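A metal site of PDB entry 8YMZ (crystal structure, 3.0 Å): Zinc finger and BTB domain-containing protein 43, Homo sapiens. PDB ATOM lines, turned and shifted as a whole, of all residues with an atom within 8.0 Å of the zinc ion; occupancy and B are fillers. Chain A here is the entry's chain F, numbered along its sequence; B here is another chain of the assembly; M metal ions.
The side-chain sulfur (SD) of Met 20 sits close to the side-chain sulfur (SG) of Cys 4, at 3.6 Å.
SG of Cys 6 of chain A lies close to N of Lys 8 (3.5 Å).
Gln 5 touches the zinc ion.
The nearest printed residue that does not touch the zinc ion is Phe 10 (5.1 Å).
The zinc ion is bound by a ring nitrogen (NE2) of His 23 (1.9 Å), a ring nitrogen (ND1) of His 19 (2.4 Å), the side-chain sulfur (SG) of Cys 4 (2.4 Å) and the side-chain sulfur (SG) of Cys 6 of chain A (2.6 Å).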
ATOM      1  N   PRO A   3       4.534  15.262  -1.516  1.00  0.00           N
ATOM      2  CA  PRO A   3       3.150  15.526  -1.115  1.00  0.00           C
ATOM      3  C   PRO A   3       2.123  14.922  -2.063  1.00  0.00           C
ATOM      4  O   PRO A   3       2.435  14.501  -3.179  1.00  0.00           O
ATOM      5  CB  PRO A   3       3.070  17.059  -1.119  1.00  0.00           C
ATOM      6  CG  PRO A   3       4.098  17.484  -2.128  1.00  0.00           C
ATOM      7  CD  PRO A   3       5.193  16.450  -2.076  1.00  0.00           C
ATOM      8  N   CYS A   4       0.874  14.834  -1.560  1.00  0.00           N
ATOM      9  CA  CYS A   4      -0.289  14.290  -2.255  1.00  0.00           C
ATOM     10  C   CYS A   4      -1.481  15.229  -2.085  1.00  0.00           C
ATOM     11  O   CYS A   4      -1.362  16.276  -1.443  1.00  0.00           O
ATOM     12  CB  CYS A   4      -0.640  12.901  -1.755  1.00  0.00           C
ATOM     13  SG  CYS A   4      -2.050  12.058  -2.522  1.00  0.00           S
ATOM     14  N   GLN A   5      -2.618  14.895  -2.698  1.00  0.00           N
ATOM     15  CA  GLN A   5      -3.791  15.790  -2.679  1.00  0.00           C
ATOM     16  C   GLN A   5      -4.617  15.608  -1.390  1.00  0.00           C
ATOM     17  O   GLN A   5      -5.779  16.010  -1.334  1.00  0.00           O
ATOM     18  CB  GLN A   5      -4.663  15.582  -3.953  1.00  0.00           C
ATOM     19  CG  GLN A   5      -4.628  16.586  -5.010  1.00  0.00           C
ATOM     20  CD  GLN A   5      -5.163  17.969  -4.504  1.00  0.00           C
ATOM     21  OE1 GLN A   5      -4.512  19.037  -4.659  1.00  0.00           O
ATOM     22  NE2 GLN A   5      -6.304  17.911  -3.735  1.00  0.00           N
ATOM     23  N   CYS A   6      -3.972  15.150  -0.325  1.00  0.00           N
ATOM     24  CA  CYS A   6      -4.644  15.036   0.965  1.00  0.00           C
ATOM     25  C   CYS A   6      -3.971  15.856   2.061  1.00  0.00           C
ATOM     26  O   CYS A   6      -4.490  15.953   3.184  1.00  0.00           O
ATOM     27  CB  CYS A   6      -4.701  13.557   1.368  1.00  0.00           C
ATOM     28  SG  CYS A   6      -3.089  12.756   1.407  1.00  0.00           S
ATOM     29  N   GLY A   7      -2.840  16.477   1.742  1.00  0.00           N
ATOM     30  CA  GLY A   7      -2.051  17.176   2.702  1.00  0.00           C
ATOM     31  C   GLY A   7      -0.962  16.337   3.311  1.00  0.00           C
ATOM     32  O   GLY A   7      -0.016  16.885   3.898  1.00  0.00           O
ATOM     33  N   LYS A   8      -1.062  15.021   3.193  1.00  0.00           N
ATOM     34  CA  LYS A   8      -0.039  14.122   3.679  1.00  0.00           C
ATOM     35  C   LYS A   8       1.129  14.132   2.694  1.00  0.00           C
ATOM     36  O   LYS A   8       0.964  13.800   1.517  1.00  0.00           O
ATOM     37  CB  LYS A   8      -0.606  12.709   3.844  1.00  0.00           C
ATOM     38  CG  LYS A   8      -0.232  12.031   5.142  1.00  0.00           C
ATOM     39  CD  LYS A   8      -0.271  10.525   4.980  1.00  0.00           C
ATOM     40  CE  LYS A   8       0.681   9.814   5.941  1.00  0.00           C
ATOM     41  NZ  LYS A   8       0.367   8.368   6.053  1.00  0.00           N
ATOM     42  N   SER A   9       2.297  14.520   3.186  1.00  0.00           N
ATOM     43  CA  SER A   9       3.516  14.491   2.381  1.00  0.00           C
ATOM     44  C   SER A   9       4.250  13.197   2.709  1.00  0.00           C
ATOM     45  O   SER A   9       4.794  13.040   3.810  1.00  0.00           O
ATOM     46  CB  SER A   9       4.403  15.708   2.656  1.00  0.00           C
ATOM     47  OG  SER A   9       5.350  15.438   3.673  1.00  0.00           O
ATOM     48  N   PHE A  10       4.247  12.279   1.755  1.00  0.00           N
ATOM     49  CA  PHE A  10       4.850  10.984   1.987  1.00  0.00           C
ATOM     50  C   PHE A  10       6.358  11.070   1.865  1.00  0.00           C
ATOM     51  O   PHE A  10       6.902  11.871   1.099  1.00  0.00           O
ATOM     52  CB  PHE A  10       4.333   9.948   0.997  1.00  0.00           C
ATOM     53  CG  PHE A  10       2.889   9.586   1.181  1.00  0.00           C
ATOM     54  CD1 PHE A  10       1.892  10.318   0.538  1.00  0.00           C
ATOM     55  CD2 PHE A  10       2.526   8.525   1.985  1.00  0.00           C
ATOM     56  CE1 PHE A  10       0.564   9.983   0.701  1.00  0.00           C
ATOM     57  CE2 PHE A  10       1.188   8.189   2.150  1.00  0.00           C
ATOM     58  CZ  PHE A  10       0.213   8.922   1.514  1.00  0.00           C
ATOM     59  N   GLN A  15       4.862   5.479  -2.360  1.00  0.00           N
ATOM     60  CA  GLN A  15       3.782   5.500  -1.378  1.00  0.00           C
ATOM     61  C   GLN A  15       2.804   6.600  -1.736  1.00  0.00           C
ATOM     62  O   GLN A  15       1.573   6.419  -1.697  1.00  0.00           O
ATOM     63  CB  GLN A  15       4.382   5.736   0.005  1.00  0.00           C
ATOM     64  CG  GLN A  15       3.818   4.926   1.140  1.00  0.00           C
ATOM     65  CD  GLN A  15       4.138   3.433   1.036  1.00  0.00           C
ATOM     66  OE1 GLN A  15       4.645   2.947   0.019  1.00  0.00           O
ATOM     67  NE2 GLN A  15       3.859   2.709   2.115  1.00  0.00           N
ATOM     68  N   ARG A  16       3.349   7.719  -2.191  1.00  0.00           N
ATOM     69  CA  ARG A  16       2.556   8.817  -2.716  1.00  0.00           C
ATOM     70  C   ARG A  16       1.745   8.361  -3.922  1.00  0.00           C
ATOM     71  O   ARG A  16       0.554   8.666  -4.037  1.00  0.00           O
ATOM     72  CB  ARG A  16       3.522   9.962  -3.051  1.00  0.00           C
ATOM     73  CG  ARG A  16       2.990  11.279  -3.598  1.00  0.00           C
ATOM     74  CD  ARG A  16       2.375  11.081  -4.970  1.00  0.00           C
ATOM     75  NE  ARG A  16       1.834  12.315  -5.522  1.00  0.00           N
ATOM     76  CZ  ARG A  16       2.574  13.201  -6.166  1.00  0.00           C
ATOM     77  NH1 ARG A  16       2.120  14.401  -6.452  1.00  0.00           N
ATOM     78  NH2 ARG A  16       3.812  12.861  -6.530  1.00  0.00           N
ATOM     79  N   ARG A  18       0.815   5.317  -4.742  1.00  0.00           N
ATOM     80  CA  ARG A  18      -0.238   4.414  -4.293  1.00  0.00           C
ATOM     81  C   ARG A  18      -1.427   5.202  -3.749  1.00  0.00           C
ATOM     82  O   ARG A  18      -2.585   4.917  -4.105  1.00  0.00           O
ATOM     83  CB  ARG A  18       0.338   3.472  -3.224  1.00  0.00           C
ATOM     84  CG  ARG A  18      -0.500   2.238  -2.937  1.00  0.00           C
ATOM     85  CD  ARG A  18       0.146   1.410  -1.838  1.00  0.00           C
ATOM     86  NE  ARG A  18       0.077   2.073  -0.546  1.00  0.00           N
ATOM     87  CZ  ARG A  18       0.414   1.519   0.609  1.00  0.00           C
ATOM     88  NH1 ARG A  18       0.864   0.278   0.677  1.00  0.00           N
ATOM     89  NH2 ARG A  18       0.286   2.226   1.735  1.00  0.00           N
ATOM     90  N   HIS A  19      -1.156   6.221  -2.927  1.00  0.00           N
ATOM     91  CA  HIS A  19      -2.239   7.071  -2.424  1.00  0.00           C
ATOM     92  C   HIS A  19      -2.975   7.755  -3.566  1.00  0.00           C
ATOM     93  O   HIS A  19      -4.220   7.785  -3.593  1.00  0.00           O
ATOM     94  CB  HIS A  19      -1.679   8.118  -1.463  1.00  0.00           C
ATOM     95  CG  HIS A  19      -2.606   8.452  -0.343  1.00  0.00           C
ATOM     96  ND1 HIS A  19      -3.015   9.738  -0.065  1.00  0.00           N
ATOM     97  CD2 HIS A  19      -3.205   7.661   0.573  1.00  0.00           C
ATOM     98  CE1 HIS A  19      -3.823   9.722   0.973  1.00  0.00           C
ATOM     99  NE2 HIS A  19      -3.956   8.472   1.381  1.00  0.00           N
ATOM    100  N   MET A  20      -2.222   8.286  -4.532  1.00  0.00           N
ATOM    101  CA  MET A  20      -2.823   8.981  -5.660  1.00  0.00           C
ATOM    102  C   MET A  20      -3.666   8.033  -6.515  1.00  0.00           C
ATOM    103  O   MET A  20      -4.781   8.371  -6.902  1.00  0.00           O
ATOM    104  CB  MET A  20      -1.725   9.641  -6.497  1.00  0.00           C
ATOM    105  CG  MET A  20      -1.525  11.103  -6.171  1.00  0.00           C
ATOM    106  SD  MET A  20      -3.097  11.953  -5.967  1.00  0.00           S
ATOM    107  CE  MET A  20      -3.133  12.932  -7.464  1.00  0.00           C
ATOM    108  N   SER A  21      -3.148   6.843  -6.797  1.00  0.00           N
ATOM    109  CA  SER A  21      -3.896   5.880  -7.592  1.00  0.00           C
ATOM    110  C   SER A  21      -5.192   5.516  -6.908  1.00  0.00           C
ATOM    111  O   SER A  21      -6.238   5.399  -7.568  1.00  0.00           O
ATOM    112  CB  SER A  21      -3.052   4.632  -7.835  1.00  0.00           C
ATOM    113  OG  SER A  21      -3.435   3.618  -6.932  1.00  0.00           O
ATOM    114  N   MET A  22      -5.157   5.343  -5.581  1.00  0.00           N
ATOM    115  CA  MET A  22      -6.393   5.101  -4.862  1.00  0.00           C
ATOM    116  C   MET A  22      -7.350   6.266  -5.011  1.00  0.00           C
ATOM    117  O   MET A  22      -8.555   6.066  -5.223  1.00  0.00           O
ATOM    118  CB  MET A  22      -6.119   4.826  -3.391  1.00  0.00           C
ATOM    119  CG  MET A  22      -7.311   5.099  -2.518  1.00  0.00           C
ATOM    120  SD  MET A  22      -6.800   5.239  -0.821  1.00  0.00           S
ATOM    121  CE  MET A  22      -6.211   6.931  -0.805  1.00  0.00           C
ATOM    122  N   HIS A  23      -6.842   7.508  -4.918  1.00  0.00           N
ATOM    123  CA  HIS A  23      -7.707   8.675  -5.118  1.00  0.00           C
ATOM    124  C   HIS A  23      -8.381   8.612  -6.479  1.00  0.00           C
ATOM    125  O   HIS A  23      -9.588   8.885  -6.597  1.00  0.00           O
ATOM    126  CB  HIS A  23      -6.898   9.969  -5.029  1.00  0.00           C
ATOM    127  CG  HIS A  23      -6.217  10.190  -3.719  1.00  0.00           C
ATOM    128  ND1 HIS A  23      -6.839   9.987  -2.512  1.00  0.00           N
ATOM    129  CD2 HIS A  23      -4.958  10.605  -3.431  1.00  0.00           C
ATOM    130  CE1 HIS A  23      -5.993  10.264  -1.532  1.00  0.00           C
ATOM    131  NE2 HIS A  23      -4.845  10.638  -2.065  1.00  0.00           N
ATOM    132  P    DT B   6      -5.140   4.414   2.932  1.00  0.00           P
ATOM    133  OP1  DT B   6      -5.547   5.781   3.343  1.00  0.00           O
ATOM    134  OP2  DT B   6      -4.345   4.196   1.700  1.00  0.00           O
ATOM    135  O5'  DT B   6      -4.293   3.793   4.115  1.00  0.00           O
ATOM    136  C5'  DT B   6      -4.980   3.180   5.195  1.00  0.00           C
ATOM    137  C4'  DT B   6      -4.002   2.758   6.255  1.00  0.00           C
ATOM    138  O4'  DT B   6      -3.755   1.333   6.141  1.00  0.00           O
ATOM    139  C3'  DT B   6      -2.637   3.421   6.166  1.00  0.00           C
ATOM    140  O3'  DT B   6      -2.071   3.499   7.459  1.00  0.00           O
ATOM    141  C2'  DT B   6      -1.861   2.431   5.293  1.00  0.00           C
ATOM    142  C1'  DT B   6      -2.390   1.116   5.838  1.00  0.00           C
ATOM    143  N1   DT B   6      -2.335   0.038   4.846  1.00  0.00           N
ATOM    144  C2   DT B   6      -2.032  -1.229   5.257  1.00  0.00           C
ATOM    145  O2   DT B   6      -1.785  -1.524   6.415  1.00  0.00           O
ATOM    146  N3   DT B   6      -2.023  -2.162   4.244  1.00  0.00           N
ATOM    147  C4   DT B   6      -2.281  -1.940   2.915  1.00  0.00           C
ATOM    148  O4   DT B   6      -2.242  -2.841   2.081  1.00  0.00           O
ATOM    149  C5   DT B   6      -2.597  -0.584   2.559  1.00  0.00           C
ATOM    150  C7   DT B   6      -2.904  -0.214   1.147  1.00  0.00           C
ATOM    151  C6   DT B   6      -2.620   0.325   3.537  1.00  0.00           C
HETATM  152 ZN    ZN M   1      -3.870  11.814  -0.939  1.00  0.00          ZN
